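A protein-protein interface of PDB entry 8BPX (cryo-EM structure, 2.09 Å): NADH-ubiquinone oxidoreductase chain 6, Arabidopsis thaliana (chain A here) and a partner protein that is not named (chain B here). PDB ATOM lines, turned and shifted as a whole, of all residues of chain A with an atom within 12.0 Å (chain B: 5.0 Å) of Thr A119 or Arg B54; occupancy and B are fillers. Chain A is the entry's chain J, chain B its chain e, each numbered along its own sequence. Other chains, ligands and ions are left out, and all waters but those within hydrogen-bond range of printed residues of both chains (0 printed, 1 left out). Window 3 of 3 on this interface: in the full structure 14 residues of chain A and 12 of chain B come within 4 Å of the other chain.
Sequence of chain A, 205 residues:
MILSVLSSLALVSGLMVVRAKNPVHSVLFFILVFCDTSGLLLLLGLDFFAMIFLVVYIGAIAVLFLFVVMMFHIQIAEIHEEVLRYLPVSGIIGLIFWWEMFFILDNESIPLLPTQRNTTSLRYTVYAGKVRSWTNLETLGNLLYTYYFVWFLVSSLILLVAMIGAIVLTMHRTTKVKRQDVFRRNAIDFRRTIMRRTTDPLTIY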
ATOM      1  N   ILE A 110     -15.201 -17.726   8.144  1.00  0.00           N
ATOM      2  CA  ILE A 110     -15.116 -16.399   8.756  1.00  0.00           C
ATOM      3  C   ILE A 110     -15.992 -16.378  10.005  1.00  0.00           C
ATOM      4  O   ILE A 110     -17.176 -16.733   9.927  1.00  0.00           O
ATOM      5  CB  ILE A 110     -15.547 -15.326   7.762  1.00  0.00           C
ATOM      6  CG1 ILE A 110     -14.491 -15.171   6.669  1.00  0.00           C
ATOM      7  CG2 ILE A 110     -15.776 -14.000   8.471  1.00  0.00           C
ATOM      8  CD1 ILE A 110     -15.024 -14.628   5.387  1.00  0.00           C
ATOM      9  N   PRO A 111     -15.460 -15.981  11.155  1.00  0.00           N
ATOM     10  CA  PRO A 111     -16.263 -15.989  12.380  1.00  0.00           C
ATOM     11  C   PRO A 111     -17.382 -14.961  12.343  1.00  0.00           C
ATOM     12  O   PRO A 111     -17.278 -13.906  11.715  1.00  0.00           O
ATOM     13  CB  PRO A 111     -15.246 -15.659  13.475  1.00  0.00           C
ATOM     14  CG  PRO A 111     -14.170 -14.924  12.779  1.00  0.00           C
ATOM     15  CD  PRO A 111     -14.090 -15.500  11.393  1.00  0.00           C
ATOM     16  N   LEU A 112     -18.468 -15.292  13.033  1.00  0.00           N
ATOM     17  CA  LEU A 112     -19.560 -14.355  13.244  1.00  0.00           C
ATOM     18  C   LEU A 112     -19.245 -13.494  14.462  1.00  0.00           C
ATOM     19  O   LEU A 112     -19.166 -14.005  15.583  1.00  0.00           O
ATOM     20  CB  LEU A 112     -20.873 -15.109  13.435  1.00  0.00           C
ATOM     21  CG  LEU A 112     -22.159 -14.291  13.508  1.00  0.00           C
ATOM     22  CD1 LEU A 112     -22.478 -13.650  12.163  1.00  0.00           C
ATOM     23  CD2 LEU A 112     -23.309 -15.158  13.986  1.00  0.00           C
ATOM     24  N   LEU A 113     -19.056 -12.198  14.245  1.00  0.00           N
ATOM     25  CA  LEU A 113     -18.769 -11.299  15.357  1.00  0.00           C
ATOM     26  C   LEU A 113     -20.004 -11.164  16.242  1.00  0.00           C
ATOM     27  O   LEU A 113     -21.091 -10.859  15.739  1.00  0.00           O
ATOM     28  CB  LEU A 113     -18.321  -9.931  14.847  1.00  0.00           C
ATOM     29  CG  LEU A 113     -17.165  -9.969  13.846  1.00  0.00           C
ATOM     30  CD1 LEU A 113     -16.797  -8.579  13.370  1.00  0.00           C
ATOM     31  CD2 LEU A 113     -15.960 -10.663  14.463  1.00  0.00           C
ATOM     32  N   PRO A 114     -19.883 -11.381  17.551  1.00  0.00           N
ATOM     33  CA  PRO A 114     -21.058 -11.299  18.433  1.00  0.00           C
ATOM     34  C   PRO A 114     -21.460  -9.847  18.648  1.00  0.00           C
ATOM     35  O   PRO A 114     -20.660  -9.030  19.106  1.00  0.00           O
ATOM     36  CB  PRO A 114     -20.573 -11.956  19.730  1.00  0.00           C
ATOM     37  CG  PRO A 114     -19.099 -11.730  19.732  1.00  0.00           C
ATOM     38  CD  PRO A 114     -18.640 -11.633  18.299  1.00  0.00           C
ATOM     39  N   THR A 115     -22.705  -9.533  18.313  1.00  0.00           N
ATOM     40  CA  THR A 115     -23.198  -8.166  18.315  1.00  0.00           C
ATOM     41  C   THR A 115     -23.968  -7.865  19.596  1.00  0.00           C
ATOM     42  O   THR A 115     -24.287  -8.753  20.390  1.00  0.00           O
ATOM     43  CB  THR A 115     -24.088  -7.917  17.093  1.00  0.00           C
ATOM     44  OG1 THR A 115     -25.253  -8.748  17.169  1.00  0.00           O
ATOM     45  CG2 THR A 115     -23.332  -8.237  15.819  1.00  0.00           C
ATOM     46  N   GLN A 116     -24.266  -6.579  19.790  1.00  0.00           N
ATOM     47  CA  GLN A 116     -25.063  -6.145  20.930  1.00  0.00           C
ATOM     48  C   GLN A 116     -26.546  -6.269  20.606  1.00  0.00           C
ATOM     49  O   GLN A 116     -27.315  -5.319  20.783  1.00  0.00           O
ATOM     50  CB  GLN A 116     -24.715  -4.706  21.317  1.00  0.00           C
ATOM     51  CG  GLN A 116     -23.246  -4.492  21.646  1.00  0.00           C
ATOM     52  CD  GLN A 116     -22.856  -5.095  22.981  1.00  0.00           C
ATOM     53  OE1 GLN A 116     -23.677  -5.200  23.891  1.00  0.00           O
ATOM     54  NE2 GLN A 116     -21.595  -5.494  23.104  1.00  0.00           N
ATOM     55  N   ARG A 117     -26.947  -7.443  20.129  1.00  0.00           N
ATOM     56  CA  ARG A 117     -28.331  -7.742  19.806  1.00  0.00           C
ATOM     57  C   ARG A 117     -28.562  -9.222  20.064  1.00  0.00           C
ATOM     58  O   ARG A 117     -27.666 -10.046  19.869  1.00  0.00           O
ATOM     59  CB  ARG A 117     -28.669  -7.391  18.357  1.00  0.00           C
ATOM     60  CG  ARG A 117     -30.111  -6.970  18.136  1.00  0.00           C
ATOM     61  CD  ARG A 117     -30.649  -7.512  16.826  1.00  0.00           C
ATOM     62  NE  ARG A 117     -31.997  -7.030  16.553  1.00  0.00           N
ATOM     63  CZ  ARG A 117     -33.100  -7.736  16.760  1.00  0.00           C
ATOM     64  NH1 ARG A 117     -33.052  -8.965  17.246  1.00  0.00           N
ATOM     65  NH2 ARG A 117     -34.280  -7.195  16.475  1.00  0.00           N
ATOM     66  N   ASN A 118     -29.767  -9.551  20.511  1.00  0.00           N
ATOM     67  CA  ASN A 118     -30.100 -10.932  20.841  1.00  0.00           C
ATOM     68  C   ASN A 118     -30.421 -11.677  19.552  1.00  0.00           C
ATOM     69  O   ASN A 118     -31.547 -11.627  19.052  1.00  0.00           O
ATOM     70  CB  ASN A 118     -31.265 -10.987  21.821  1.00  0.00           C
ATOM     71  CG  ASN A 118     -31.369 -12.324  22.521  1.00  0.00           C
ATOM     72  OD1 ASN A 118     -30.358 -12.953  22.836  1.00  0.00           O
ATOM     73  ND2 ASN A 118     -32.595 -12.770  22.769  1.00  0.00           N
ATOM     74  N   THR A 119     -29.423 -12.374  19.010  1.00  0.00           N
ATOM     75  CA  THR A 119     -29.633 -13.235  17.855  1.00  0.00           C
ATOM     76  C   THR A 119     -30.268 -14.568  18.232  1.00  0.00           C
ATOM     77  O   THR A 119     -30.689 -15.312  17.339  1.00  0.00           O
ATOM     78  CB  THR A 119     -28.303 -13.477  17.133  1.00  0.00           C
ATOM     79  OG1 THR A 119     -27.505 -12.289  17.194  1.00  0.00           O
ATOM     80  CG2 THR A 119     -28.538 -13.830  15.670  1.00  0.00           C
ATOM     81  N   THR A 120     -30.363 -14.876  19.530  1.00  0.00           N
ATOM     82  CA  THR A 120     -30.916 -16.158  19.956  1.00  0.00           C
ATOM     83  C   THR A 120     -32.354 -16.342  19.487  1.00  0.00           C
ATOM     84  O   THR A 120     -32.797 -17.477  19.280  1.00  0.00           O
ATOM     85  CB  THR A 120     -30.842 -16.286  21.478  1.00  0.00           C
ATOM     86  OG1 THR A 120     -31.690 -15.304  22.085  1.00  0.00           O
ATOM     87  CG2 THR A 120     -29.412 -16.086  21.960  1.00  0.00           C
ATOM     88  N   SER A 121     -33.091 -15.248  19.297  1.00  0.00           N
ATOM     89  CA  SER A 121     -34.470 -15.360  18.841  1.00  0.00           C
ATOM     90  C   SER A 121     -34.565 -15.806  17.388  1.00  0.00           C
ATOM     91  O   SER A 121     -35.630 -16.261  16.963  1.00  0.00           O
ATOM     92  CB  SER A 121     -35.193 -14.028  19.020  1.00  0.00           C
ATOM     93  OG  SER A 121     -35.131 -13.257  17.835  1.00  0.00           O
ATOM     94  N   LEU A 122     -33.485 -15.690  16.621  1.00  0.00           N
ATOM     95  CA  LEU A 122     -33.475 -16.124  15.233  1.00  0.00           C
ATOM     96  C   LEU A 122     -33.115 -17.593  15.072  1.00  0.00           C
ATOM     97  O   LEU A 122     -33.035 -18.075  13.938  1.00  0.00           O
ATOM     98  CB  LEU A 122     -32.517 -15.255  14.413  1.00  0.00           C
ATOM     99  CG  LEU A 122     -33.003 -13.821  14.184  1.00  0.00           C
ATOM    100  CD1 LEU A 122     -32.276 -13.179  13.020  1.00  0.00           C
ATOM    101  CD2 LEU A 122     -34.502 -13.806  13.940  1.00  0.00           C
ATOM    102  N   ARG A 123     -32.890 -18.308  16.170  1.00  0.00           N
ATOM    103  CA  ARG A 123     -32.704 -19.750  16.100  1.00  0.00           C
ATOM    104  C   ARG A 123     -34.028 -20.412  15.730  1.00  0.00           C
ATOM    105  O   ARG A 123     -35.020 -20.278  16.453  1.00  0.00           O
ATOM    106  CB  ARG A 123     -32.186 -20.284  17.435  1.00  0.00           C
ATOM    107  CG  ARG A 123     -31.046 -21.282  17.306  1.00  0.00           C
ATOM    108  CD  ARG A 123     -30.093 -21.212  18.491  1.00  0.00           C
ATOM    109  NE  ARG A 123     -29.220 -20.046  18.430  1.00  0.00           N
ATOM    110  CZ  ARG A 123     -28.372 -19.694  19.387  1.00  0.00           C
ATOM    111  NH1 ARG A 123     -28.251 -20.402  20.498  1.00  0.00           N
ATOM    112  NH2 ARG A 123     -27.624 -18.607  19.223  1.00  0.00           N
ATOM    113  N   TYR A 124     -34.046 -21.114  14.603  1.00  0.00           N
ATOM    114  CA  TYR A 124     -35.243 -21.798  14.131  1.00  0.00           C
ATOM    115  C   TYR A 124     -35.231 -23.242  14.616  1.00  0.00           C
ATOM    116  O   TYR A 124     -34.237 -23.951  14.441  1.00  0.00           O
ATOM    117  CB  TYR A 124     -35.321 -21.747  12.604  1.00  0.00           C
ATOM    118  CG  TYR A 124     -36.567 -22.376  12.023  1.00  0.00           C
ATOM    119  CD1 TYR A 124     -37.829 -22.018  12.483  1.00  0.00           C
ATOM    120  CD2 TYR A 124     -36.483 -23.328  11.016  1.00  0.00           C
ATOM    121  CE1 TYR A 124     -38.966 -22.587  11.958  1.00  0.00           C
ATOM    122  CE2 TYR A 124     -37.617 -23.905  10.486  1.00  0.00           C
ATOM    123  CZ  TYR A 124     -38.856 -23.532  10.961  1.00  0.00           C
ATOM    124  OH  TYR A 124     -39.984 -24.105  10.436  1.00  0.00           O
ATOM    125  N   THR A 125     -36.335 -23.674  15.219  1.00  0.00           N
ATOM    126  CA  THR A 125     -36.456 -25.015  15.779  1.00  0.00           C
ATOM    127  C   THR A 125     -37.327 -25.873  14.871  1.00  0.00           C
ATOM    128  O   THR A 125     -38.464 -25.502  14.564  1.00  0.00           O
ATOM    129  CB  THR A 125     -37.047 -24.969  17.188  1.00  0.00           C
ATOM    130  OG1 THR A 125     -36.105 -24.360  18.079  1.00  0.00           O
ATOM    131  CG2 THR A 125     -37.377 -26.366  17.679  1.00  0.00           C
ATOM    132  N   LYS B  49     -20.115 -16.305   3.331  1.00  0.00           N
ATOM    133  CA  LYS B  49     -20.727 -15.067   2.854  1.00  0.00           C
ATOM    134  C   LYS B  49     -21.793 -14.559   3.817  1.00  0.00           C
ATOM    135  O   LYS B  49     -21.919 -13.345   4.027  1.00  0.00           O
ATOM    136  CB  LYS B  49     -21.297 -15.260   1.450  1.00  0.00           C
ATOM    137  CG  LYS B  49     -20.230 -15.501   0.394  1.00  0.00           C
ATOM    138  CD  LYS B  49     -20.806 -15.913  -0.956  1.00  0.00           C
ATOM    139  CE  LYS B  49     -22.010 -16.811  -0.832  1.00  0.00           C
ATOM    140  NZ  LYS B  49     -21.586 -18.218  -0.666  1.00  0.00           N
ATOM    141  N   GLU B  50     -22.565 -15.469   4.412  1.00  0.00           N
ATOM    142  CA  GLU B  50     -23.558 -15.081   5.410  1.00  0.00           C
ATOM    143  C   GLU B  50     -22.910 -14.328   6.566  1.00  0.00           C
ATOM    144  O   GLU B  50     -23.341 -13.225   6.934  1.00  0.00           O
ATOM    145  CB  GLU B  50     -24.279 -16.329   5.924  1.00  0.00           C
ATOM    146  CG  GLU B  50     -25.716 -16.110   6.366  1.00  0.00           C
ATOM    147  CD  GLU B  50     -26.246 -17.250   7.221  1.00  0.00           C
ATOM    148  OE1 GLU B  50     -26.352 -18.385   6.710  1.00  0.00           O
ATOM    149  OE2 GLU B  50     -26.577 -17.011   8.399  1.00  0.00           O
ATOM    150  N   PHE B  51     -21.857 -14.910   7.140  1.00  0.00           N
ATOM    151  CA  PHE B  51     -21.188 -14.290   8.276  1.00  0.00           C
ATOM    152  C   PHE B  51     -20.486 -13.001   7.866  1.00  0.00           C
ATOM    153  O   PHE B  51     -20.450 -12.041   8.638  1.00  0.00           O
ATOM    154  CB  PHE B  51     -20.205 -15.279   8.908  1.00  0.00           C
ATOM    155  CG  PHE B  51     -20.874 -16.434   9.609  1.00  0.00           C
ATOM    156  CD1 PHE B  51     -22.237 -16.420   9.848  1.00  0.00           C
ATOM    157  CD2 PHE B  51     -20.141 -17.531  10.031  1.00  0.00           C
ATOM    158  CE1 PHE B  51     -22.857 -17.472  10.485  1.00  0.00           C
ATOM    159  CE2 PHE B  51     -20.756 -18.590  10.672  1.00  0.00           C
ATOM    160  CZ  PHE B  51     -22.112 -18.563  10.900  1.00  0.00           C
ATOM    161  N   GLN B  52     -19.934 -12.955   6.651  1.00  0.00           N
ATOM    162  CA  GLN B  52     -19.312 -11.725   6.171  1.00  0.00           C
ATOM    163  C   GLN B  52     -20.328 -10.589   6.079  1.00  0.00           C
ATOM    164  O   GLN B  52     -20.052  -9.458   6.499  1.00  0.00           O
ATOM    165  CB  GLN B  52     -18.662 -11.967   4.811  1.00  0.00           C
ATOM    166  CG  GLN B  52     -17.884 -10.783   4.278  1.00  0.00           C
ATOM    167  CD  GLN B  52     -16.631 -11.205   3.546  1.00  0.00           C
ATOM    168  OE1 GLN B  52     -16.370 -12.394   3.369  1.00  0.00           O
ATOM    169  NE2 GLN B  52     -15.838 -10.230   3.132  1.00  0.00           N
ATOM    170  N   ARG B  53     -21.511 -10.872   5.531  1.00  0.00           N
ATOM    171  CA  ARG B  53     -22.551  -9.852   5.418  1.00  0.00           C
ATOM    172  C   ARG B  53     -23.031  -9.395   6.794  1.00  0.00           C
ATOM    173  O   ARG B  53     -23.212  -8.191   7.043  1.00  0.00           O
ATOM    174  CB  ARG B  53     -23.706 -10.404   4.582  1.00  0.00           C
ATOM    175  CG  ARG B  53     -25.052  -9.755   4.826  1.00  0.00           C
ATOM    176  CD  ARG B  53     -26.115 -10.408   3.963  1.00  0.00           C
ATOM    177  NE  ARG B  53     -27.377  -9.681   4.004  1.00  0.00           N
ATOM    178  CZ  ARG B  53     -27.715  -8.730   3.144  1.00  0.00           C
ATOM    179  NH1 ARG B  53     -26.899  -8.361   2.170  1.00  0.00           N
ATOM    180  NH2 ARG B  53     -28.897  -8.136   3.268  1.00  0.00           N
ATOM    181  N   ARG B  54     -23.240 -10.344   7.710  1.00  0.00           N
ATOM    182  CA  ARG B  54     -23.648  -9.962   9.058  1.00  0.00           C
ATOM    183  C   ARG B  54     -22.569  -9.142   9.758  1.00  0.00           C
ATOM    184  O   ARG B  54     -22.882  -8.219  10.523  1.00  0.00           O
ATOM    185  CB  ARG B  54     -24.009 -11.206   9.869  1.00  0.00           C
ATOM    186  CG  ARG B  54     -25.448 -11.639   9.663  1.00  0.00           C
ATOM    187  CD  ARG B  54     -25.662 -13.130   9.868  1.00  0.00           C
ATOM    188  NE  ARG B  54     -26.068 -13.449  11.231  1.00  0.00           N
ATOM    189  CZ  ARG B  54     -26.360 -14.669  11.659  1.00  0.00           C
ATOM    190  NH1 ARG B  54     -26.342 -15.713  10.845  1.00  0.00           N
ATOM    191  NH2 ARG B  54     -26.680 -14.848  12.936  1.00  0.00           N
ATOM    192  N   ASN B  55     -21.296  -9.444   9.493  1.00  0.00           N
ATOM    193  CA  ASN B  55     -20.216  -8.645  10.055  1.00  0.00           C
ATOM    194  C   ASN B  55     -20.187  -7.250   9.453  1.00  0.00           C
ATOM    195  O   ASN B  55     -19.828  -6.295  10.141  1.00  0.00           O
ATOM    196  CB  ASN B  55     -18.875  -9.344   9.847  1.00  0.00           C
ATOM    197  CG  ASN B  55     -18.725 -10.584  10.712  1.00  0.00           C
ATOM    198  OD1 ASN B  55     -19.489 -10.793  11.653  1.00  0.00           O
ATOM    199  ND2 ASN B  55     -17.736 -11.408  10.398  1.00  0.00           N
ATOM    200  N   ARG B  56     -20.546  -7.116   8.176  1.00  0.00           N
ATOM    201  CA  ARG B  56     -20.707  -5.785   7.598  1.00  0.00           C
ATOM    202  C   ARG B  56     -21.784  -4.998   8.334  1.00  0.00           C
ATOM    203  O   ARG B  56     -21.620  -3.801   8.605  1.00  0.00           O
ATOM    204  CB  ARG B  56     -21.048  -5.889   6.112  1.00  0.00           C
ATOM    205  CG  ARG B  56     -19.900  -5.556   5.198  1.00  0.00           C
ATOM    206  CD  ARG B  56     -20.279  -5.712   3.745  1.00  0.00           C
ATOM    207  NE  ARG B  56     -19.356  -6.583   3.030  1.00  0.00           N
ATOM    208  CZ  ARG B  56     -19.611  -7.843   2.713  1.00  0.00           C
ATOM    209  NH1 ARG B  56     -20.765  -8.412   3.019  1.00  0.00           N
ATOM    210  NH2 ARG B  56     -18.689  -8.548   2.066  1.00  0.00           N
ATOM    211  N   ILE B  57     -22.895  -5.658   8.665  1.00  0.00           N
ATOM    212  CA  ILE B  57     -23.958  -4.982   9.410  1.00  0.00           C
ATOM    213  C   ILE B  57     -23.443  -4.526  10.772  1.00  0.00           C
ATOM    214  O   ILE B  57     -23.668  -3.384  11.198  1.00  0.00           O
ATOM    215  CB  ILE B  57     -25.187  -5.896   9.550  1.00  0.00           C
ATOM    216  CG1 ILE B  57     -25.916  -6.022   8.214  1.00  0.00           C
ATOM    217  CG2 ILE B  57     -26.137  -5.364  10.619  1.00  0.00           C
ATOM    218  CD1 ILE B  57     -26.782  -7.250   8.120  1.00  0.00           C
ATOM    219  N   TYR B  58     -22.731  -5.414  11.470  1.00  0.00           N
ATOM    220  CA  TYR B  58     -22.160  -5.060  12.769  1.00  0.00           C
ATOM    221  C   TYR B  58     -21.154  -3.918  12.643  1.00  0.00           C
ATOM    222  O   TYR B  58     -21.089  -3.034  13.507  1.00  0.00           O
ATOM    223  CB  TYR B  58     -21.510  -6.292  13.399  1.00  0.00           C
ATOM    224  CG  TYR B  58     -20.449  -5.995  14.437  1.00  0.00           C
ATOM    225  CD1 TYR B  58     -20.792  -5.715  15.752  1.00  0.00           C
ATOM    226  CD2 TYR B  58     -19.102  -6.003  14.101  1.00  0.00           C
ATOM    227  CE1 TYR B  58     -19.825  -5.447  16.699  1.00  0.00           C
ATOM    228  CE2 TYR B  58     -18.130  -5.735  15.043  1.00  0.00           C
ATOM    229  CZ  TYR B  58     -18.494  -5.459  16.337  1.00  0.00           C
ATOM    230  OH  TYR B  58     -17.523  -5.193  17.273  1.00  0.00           O
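Along chain B the printed residues that touch a printed residue of chain A span positions 51 to 58.
Thr A119 touches just one residue of chain B: Arg B54.
Arg B54 touches just these residues of chain A: Leu A112 and Thr A119.
No residue of chain A comes within 4 Å of Glu B50.
Of chain A, only Ile A110 and Leu A112 come within 4 Å of Phe B51.
No residue of chain A comes within 4 Å of Arg B53.
Ile B57 touches none of the printed residues of chain A.
Printed residues of chain B within 4 Å of Leu A113: Asn B55 (3.0 Å) and Tyr B58 (3.5 Å).
Printed residues of chain A within 4 Å of Gln B52: Ile A110.
Tyr A124 touches none of the printed residues of chain B.
The nearest printed residue of chain B that does not touch Thr A119 is Glu B50 (8.2 Å).
The guanidinium group of Arg B54 lies within salt-bridge range of the side-chain carboxylate of Glu B50.
O of Phe B51 lies close to ND2 of Asn B55 (3.3 Å).
The backbone carbonyl oxygen (O) of Arg A117 lies within hydrogen-bond range of the side-chain hydroxyl (OG1) of Thr A119 (3.5 Å).
The side-chain amide nitrogen (NE2) of Gln B52 lies close to the guanidinium group (NH2) of Arg B56 (3.5 Å).
Ile A110 touches Phe B51 (O to CD2, 3.1 Å).
OE1 of Gln B52 touches CD1 of Ile A110, at 3.3 Å.
Ile A110 touches Asn B55 (CG2 to ND2, 3.8 Å).
CD1 of Leu A112 touches CD1 of Phe B51, at 3.6 Å.
NH2 of Arg B54 touches CD2 of Leu A112, at 3.5 Å.
Leu A112 touches Asn B55 (CA to OD1, 3.9 Å).
CD2 of Tyr B58 touches CD1 of Leu A113, 3.5 Å away.
CD1 of Tyr B58 touches CG2 of Thr A115, at 3.6 Å.
CG2 of Thr A119 touches NH2 of Arg B54, at 3.5 Å.
O of Pro A111 sits at hydrogen-bond distance from ND2 of Asn B55 (2.9 Å).
The backbone NH (N) of Leu A113 lies within hydrogen-bond range of the side-chain amide oxygen (OD1) of Asn B55, 3.0 Å away.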
